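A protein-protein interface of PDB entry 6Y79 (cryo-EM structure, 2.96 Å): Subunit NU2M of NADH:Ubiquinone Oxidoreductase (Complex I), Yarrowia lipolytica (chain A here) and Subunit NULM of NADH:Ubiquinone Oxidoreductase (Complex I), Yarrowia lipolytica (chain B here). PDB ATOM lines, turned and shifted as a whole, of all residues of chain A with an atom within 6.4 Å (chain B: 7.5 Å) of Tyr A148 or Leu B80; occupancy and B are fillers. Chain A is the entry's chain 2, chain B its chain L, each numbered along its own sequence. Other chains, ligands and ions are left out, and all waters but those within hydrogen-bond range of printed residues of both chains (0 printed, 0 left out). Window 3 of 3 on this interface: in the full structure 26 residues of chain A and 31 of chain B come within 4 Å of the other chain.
The backbone carbonyl oxygen of Ser A147 sits at hydrogen-bond distance from the side-chain hydroxyl of Ser A151, at 2.5 Å.
The side-chain hydroxyl (OH) of Tyr B77 is in hydrogen-bond range of the backbone carbonyl oxygen (O) of Ile B89 (3.3 Å).
Of the 10 printed residues of chain B, 4 touch a printed residue of chain A.
Among the printed residues, 8 pairs touch across the chains.
Among the printed residues, no Asp or Glu carboxylate lies within 4 Å of a Lys or Arg side-chain nitrogen of the other chain.
Among the printed residues, merely in contact across the chains: Asn A145 with Leu B80 (3.2 Å), Ser A146 with Leu B80 (3.95 Å), Ser A147 with Leu B80 (3.5 Å), Tyr A148 with Leu B80 (3.6 Å), Tyr A148 with Arg B81 (3.3 Å), Ser A151 with Tyr B77 (3.96 Å), Ser A151 with Arg B81 (3.4 Å) and Lys A152 with Ile B89 (3.4 Å).
Tyr A148 touches two residues of chain B.
Leu B80 touches just these residues of chain A: Asn A145, Ser A146, Ser A147 and Tyr A148.
Of the printed residues of chain B, Asn A145 touches Leu B80.
Printed residues of chain B within 4 Å of Lys A152: Ile B89.
Of the printed residues of chain B, Ser A146 touches Leu B80.
Printed residues of chain A within 4 Å of Ile B89: Lys A152.
Printed residues of chain B within 4 Å of Ser A151: Tyr B77 (3.96 Å) and Arg B81 (3.4 Å).
Tyr B78 touches none of the printed residues of chain A.
The nearest residue of chain B that does not touch Tyr A148 is Tyr B77 (5.6 Å).
The nearest printed residue of chain A that does not touch Arg B81 is Lys A152 (4.1 Å).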
ATOM      1  N   TYR A 144     -24.575  14.240  20.544  1.00  0.00           N
ATOM      2  CA  TYR A 144     -24.224  15.405  19.737  1.00  0.00           C
ATOM      3  C   TYR A 144     -24.260  14.970  18.275  1.00  0.00           C
ATOM      4  O   TYR A 144     -23.244  14.755  17.618  1.00  0.00           O
ATOM      5  CB  TYR A 144     -22.867  15.970  20.138  1.00  0.00           C
ATOM      6  CG  TYR A 144     -22.779  16.571  21.530  1.00  0.00           C
ATOM      7  CD1 TYR A 144     -23.897  16.825  22.293  1.00  0.00           C
ATOM      8  CD2 TYR A 144     -21.566  16.897  22.068  1.00  0.00           C
ATOM      9  CE1 TYR A 144     -23.785  17.360  23.560  1.00  0.00           C
ATOM     10  CE2 TYR A 144     -21.448  17.428  23.328  1.00  0.00           C
ATOM     11  CZ  TYR A 144     -22.567  17.663  24.063  1.00  0.00           C
ATOM     12  OH  TYR A 144     -22.467  18.203  25.317  1.00  0.00           O
ATOM     13  N   ASN A 145     -25.486  14.815  17.782  1.00  0.00           N
ATOM     14  CA  ASN A 145     -25.722  14.185  16.493  1.00  0.00           C
ATOM     15  C   ASN A 145     -25.516  15.122  15.320  1.00  0.00           C
ATOM     16  O   ASN A 145     -25.661  14.682  14.181  1.00  0.00           O
ATOM     17  CB  ASN A 145     -27.139  13.603  16.433  1.00  0.00           C
ATOM     18  CG  ASN A 145     -28.208  14.616  16.799  1.00  0.00           C
ATOM     19  OD1 ASN A 145     -27.913  15.755  17.148  1.00  0.00           O
ATOM     20  ND2 ASN A 145     -29.461  14.204  16.711  1.00  0.00           N
ATOM     21  N   SER A 146     -25.210  16.393  15.559  1.00  0.00           N
ATOM     22  CA  SER A 146     -24.915  17.323  14.471  1.00  0.00           C
ATOM     23  C   SER A 146     -23.428  17.331  14.151  1.00  0.00           C
ATOM     24  O   SER A 146     -22.804  18.378  14.046  1.00  0.00           O
ATOM     25  CB  SER A 146     -25.389  18.720  14.841  1.00  0.00           C
ATOM     26  OG  SER A 146     -26.741  18.718  15.241  1.00  0.00           O
ATOM     27  N   SER A 147     -22.856  16.145  13.980  1.00  0.00           N
ATOM     28  CA  SER A 147     -21.412  15.976  13.879  1.00  0.00           C
ATOM     29  C   SER A 147     -21.167  14.670  13.153  1.00  0.00           C
ATOM     30  O   SER A 147     -21.709  13.639  13.553  1.00  0.00           O
ATOM     31  CB  SER A 147     -20.770  15.964  15.257  1.00  0.00           C
ATOM     32  OG  SER A 147     -19.378  15.769  15.165  1.00  0.00           O
ATOM     33  N   TYR A 148     -20.368  14.716  12.090  1.00  0.00           N
ATOM     34  CA  TYR A 148     -20.138  13.527  11.278  1.00  0.00           C
ATOM     35  C   TYR A 148     -19.320  12.495  12.042  1.00  0.00           C
ATOM     36  O   TYR A 148     -19.615  11.290  12.001  1.00  0.00           O
ATOM     37  CB  TYR A 148     -19.425  13.915   9.983  1.00  0.00           C
ATOM     38  CG  TYR A 148     -20.190  14.834   9.046  1.00  0.00           C
ATOM     39  CD1 TYR A 148     -21.560  14.986   9.138  1.00  0.00           C
ATOM     40  CD2 TYR A 148     -19.529  15.539   8.058  1.00  0.00           C
ATOM     41  CE1 TYR A 148     -22.244  15.821   8.287  1.00  0.00           C
ATOM     42  CE2 TYR A 148     -20.207  16.376   7.201  1.00  0.00           C
ATOM     43  CZ  TYR A 148     -21.566  16.508   7.319  1.00  0.00           C
ATOM     44  OH  TYR A 148     -22.251  17.338   6.466  1.00  0.00           O
ATOM     45  N   LYS A 149     -18.303  12.965  12.770  1.00  0.00           N
ATOM     46  CA  LYS A 149     -17.375  12.079  13.459  1.00  0.00           C
ATOM     47  C   LYS A 149     -18.037  11.376  14.631  1.00  0.00           C
ATOM     48  O   LYS A 149     -17.809  10.184  14.848  1.00  0.00           O
ATOM     49  CB  LYS A 149     -16.171  12.873  13.944  1.00  0.00           C
ATOM     50  CG  LYS A 149     -15.302  13.456  12.866  1.00  0.00           C
ATOM     51  CD  LYS A 149     -14.213  14.266  13.524  1.00  0.00           C
ATOM     52  CE  LYS A 149     -13.308  14.942  12.528  1.00  0.00           C
ATOM     53  NZ  LYS A 149     -12.144  15.544  13.237  1.00  0.00           N
ATOM     54  N   ALA A 150     -18.867  12.092  15.392  1.00  0.00           N
ATOM     55  CA  ALA A 150     -19.545  11.479  16.528  1.00  0.00           C
ATOM     56  C   ALA A 150     -20.611  10.488  16.086  1.00  0.00           C
ATOM     57  O   ALA A 150     -20.814   9.469  16.757  1.00  0.00           O
ATOM     58  CB  ALA A 150     -20.154  12.553  17.418  1.00  0.00           C
ATOM     59  N   SER A 151     -21.267  10.744  14.949  1.00  0.00           N
ATOM     60  CA  SER A 151     -22.227   9.782  14.420  1.00  0.00           C
ATOM     61  C   SER A 151     -21.526   8.505  13.970  1.00  0.00           C
ATOM     62  O   SER A 151     -21.965   7.393  14.307  1.00  0.00           O
ATOM     63  CB  SER A 151     -23.004  10.406  13.265  1.00  0.00           C
ATOM     64  OG  SER A 151     -23.381  11.742  13.554  1.00  0.00           O
ATOM     65  N   LYS A 152     -20.422   8.645  13.229  1.00  0.00           N
ATOM     66  CA  LYS A 152     -19.662   7.477  12.788  1.00  0.00           C
ATOM     67  C   LYS A 152     -19.076   6.716  13.971  1.00  0.00           C
ATOM     68  O   LYS A 152     -19.044   5.478  13.971  1.00  0.00           O
ATOM     69  CB  LYS A 152     -18.561   7.921  11.825  1.00  0.00           C
ATOM     70  CG  LYS A 152     -17.767   6.799  11.204  1.00  0.00           C
ATOM     71  CD  LYS A 152     -16.739   7.368  10.249  1.00  0.00           C
ATOM     72  CE  LYS A 152     -15.692   8.181  10.993  1.00  0.00           C
ATOM     73  NZ  LYS A 152     -14.756   7.309  11.742  1.00  0.00           N
ATOM     74  N   ALA A 153     -18.672   7.442  15.019  1.00  0.00           N
ATOM     75  CA  ALA A 153     -18.114   6.817  16.209  1.00  0.00           C
ATOM     76  C   ALA A 153     -19.169   6.047  16.984  1.00  0.00           C
ATOM     77  O   ALA A 153     -18.884   4.969  17.508  1.00  0.00           O
ATOM     78  CB  ALA A 153     -17.470   7.876  17.093  1.00  0.00           C
ATOM     79  N   VAL B  75     -30.495   5.845  12.326  1.00  0.00           N
ATOM     80  CA  VAL B  75     -31.289   6.954  11.797  1.00  0.00           C
ATOM     81  C   VAL B  75     -30.552   8.277  11.980  1.00  0.00           C
ATOM     82  O   VAL B  75     -30.501   9.104  11.062  1.00  0.00           O
ATOM     83  CB  VAL B  75     -32.686   6.969  12.446  1.00  0.00           C
ATOM     84  CG1 VAL B  75     -33.440   8.240  12.113  1.00  0.00           C
ATOM     85  CG2 VAL B  75     -33.486   5.781  11.978  1.00  0.00           C
ATOM     86  N   SER B  76     -29.900   8.465  13.132  1.00  0.00           N
ATOM     87  CA  SER B  76     -29.110   9.681  13.326  1.00  0.00           C
ATOM     88  C   SER B  76     -27.835   9.684  12.497  1.00  0.00           C
ATOM     89  O   SER B  76     -27.302  10.753  12.187  1.00  0.00           O
ATOM     90  CB  SER B  76     -28.747   9.871  14.783  1.00  0.00           C
ATOM     91  OG  SER B  76     -27.852   8.882  15.240  1.00  0.00           O
ATOM     92  N   TYR B  77     -27.294   8.502  12.185  1.00  0.00           N
ATOM     93  CA  TYR B  77     -26.210   8.428  11.211  1.00  0.00           C
ATOM     94  C   TYR B  77     -26.677   8.909   9.850  1.00  0.00           C
ATOM     95  O   TYR B  77     -25.928   9.573   9.130  1.00  0.00           O
ATOM     96  CB  TYR B  77     -25.688   6.996  11.117  1.00  0.00           C
ATOM     97  CG  TYR B  77     -24.530   6.797  10.163  1.00  0.00           C
ATOM     98  CD1 TYR B  77     -23.230   7.000  10.579  1.00  0.00           C
ATOM     99  CD2 TYR B  77     -24.739   6.380   8.851  1.00  0.00           C
ATOM    100  CE1 TYR B  77     -22.172   6.815   9.719  1.00  0.00           C
ATOM    101  CE2 TYR B  77     -23.687   6.203   7.984  1.00  0.00           C
ATOM    102  CZ  TYR B  77     -22.407   6.421   8.425  1.00  0.00           C
ATOM    103  OH  TYR B  77     -21.353   6.244   7.567  1.00  0.00           O
ATOM    104  N   TYR B  78     -27.915   8.591   9.496  1.00  0.00           N
ATOM    105  CA  TYR B  78     -28.498   8.914   8.204  1.00  0.00           C
ATOM    106  C   TYR B  78     -28.992  10.353   8.100  1.00  0.00           C
ATOM    107  O   TYR B  78     -29.185  10.831   6.981  1.00  0.00           O
ATOM    108  CB  TYR B  78     -29.648   7.936   7.940  1.00  0.00           C
ATOM    109  CG  TYR B  78     -30.331   8.053   6.606  1.00  0.00           C
ATOM    110  CD1 TYR B  78     -29.807   7.439   5.484  1.00  0.00           C
ATOM    111  CD2 TYR B  78     -31.517   8.764   6.476  1.00  0.00           C
ATOM    112  CE1 TYR B  78     -30.434   7.543   4.268  1.00  0.00           C
ATOM    113  CE2 TYR B  78     -32.143   8.878   5.266  1.00  0.00           C
ATOM    114  CZ  TYR B  78     -31.600   8.263   4.168  1.00  0.00           C
ATOM    115  OH  TYR B  78     -32.234   8.370   2.960  1.00  0.00           O
ATOM    116  N   ARG B  79     -29.209  11.043   9.228  1.00  0.00           N
ATOM    117  CA  ARG B  79     -29.739  12.410   9.205  1.00  0.00           C
ATOM    118  C   ARG B  79     -28.852  13.370   8.427  1.00  0.00           C
ATOM    119  O   ARG B  79     -29.343  14.169   7.625  1.00  0.00           O
ATOM    120  CB  ARG B  79     -29.891  12.965  10.616  1.00  0.00           C
ATOM    121  CG  ARG B  79     -30.892  12.306  11.499  1.00  0.00           C
ATOM    122  CD  ARG B  79     -30.954  13.045  12.813  1.00  0.00           C
ATOM    123  NE  ARG B  79     -31.404  14.408  12.591  1.00  0.00           N
ATOM    124  CZ  ARG B  79     -32.648  14.813  12.801  1.00  0.00           C
ATOM    125  NH1 ARG B  79     -32.984  16.067  12.560  1.00  0.00           N
ATOM    126  NH2 ARG B  79     -33.552  13.960  13.258  1.00  0.00           N
ATOM    127  N   LEU B  80     -27.549  13.316   8.662  1.00  0.00           N
ATOM    128  CA  LEU B  80     -26.627  14.261   8.060  1.00  0.00           C
ATOM    129  C   LEU B  80     -26.067  13.774   6.740  1.00  0.00           C
ATOM    130  O   LEU B  80     -25.582  14.583   5.946  1.00  0.00           O
ATOM    131  CB  LEU B  80     -25.472  14.528   9.013  1.00  0.00           C
ATOM    132  CG  LEU B  80     -25.776  15.051  10.404  1.00  0.00           C
ATOM    133  CD1 LEU B  80     -24.507  14.975  11.165  1.00  0.00           C
ATOM    134  CD2 LEU B  80     -26.266  16.476  10.343  1.00  0.00           C
ATOM    135  N   ARG B  81     -26.114  12.475   6.502  1.00  0.00           N
ATOM    136  CA  ARG B  81     -25.676  11.873   5.255  1.00  0.00           C
ATOM    137  C   ARG B  81     -26.870  11.118   4.709  1.00  0.00           C
ATOM    138  O   ARG B  81     -27.167  10.020   5.183  1.00  0.00           O
ATOM    139  CB  ARG B  81     -24.503  10.920   5.482  1.00  0.00           C
ATOM    140  CG  ARG B  81     -23.153  11.585   5.552  1.00  0.00           C
ATOM    141  CD  ARG B  81     -22.842  12.080   6.949  1.00  0.00           C
ATOM    142  NE  ARG B  81     -22.566  10.980   7.864  1.00  0.00           N
ATOM    143  CZ  ARG B  81     -22.696  11.061   9.181  1.00  0.00           C
ATOM    144  NH1 ARG B  81     -23.118  12.174   9.752  1.00  0.00           N
ATOM    145  NH2 ARG B  81     -22.416  10.024   9.929  1.00  0.00           N
ATOM    146  N   GLY B  82     -27.511  11.640   3.667  1.00  0.00           N
ATOM    147  CA  GLY B  82     -28.730  11.028   3.154  1.00  0.00           C
ATOM    148  C   GLY B  82     -28.549   9.744   2.364  1.00  0.00           C
ATOM    149  O   GLY B  82     -29.397   9.362   1.554  1.00  0.00           O
ATOM    150  N   VAL B  83     -27.438   9.067   2.623  1.00  0.00           N
ATOM    151  CA  VAL B  83     -26.998   7.876   1.931  1.00  0.00           C
ATOM    152  C   VAL B  83     -26.326   7.016   2.986  1.00  0.00           C
ATOM    153  O   VAL B  83     -25.804   7.523   3.982  1.00  0.00           O
ATOM    154  CB  VAL B  83     -26.051   8.252   0.759  1.00  0.00           C
ATOM    155  CG1 VAL B  83     -24.782   8.949   1.257  1.00  0.00           C
ATOM    156  CG2 VAL B  83     -25.698   7.058  -0.101  1.00  0.00           C
ATOM    157  N   ILE B  89     -19.729   2.074   7.298  1.00  0.00           N
ATOM    158  CA  ILE B  89     -19.724   3.382   7.931  1.00  0.00           C
ATOM    159  C   ILE B  89     -18.367   4.051   7.760  1.00  0.00           C
ATOM    160  O   ILE B  89     -18.223   5.249   8.001  1.00  0.00           O
ATOM    161  CB  ILE B  89     -20.090   3.276   9.414  1.00  0.00           C
ATOM    162  CG1 ILE B  89     -19.067   2.412  10.144  1.00  0.00           C
ATOM    163  CG2 ILE B  89     -21.487   2.707   9.583  1.00  0.00           C
ATOM    164  CD1 ILE B  89     -19.239   2.409  11.622  1.00  0.00           C
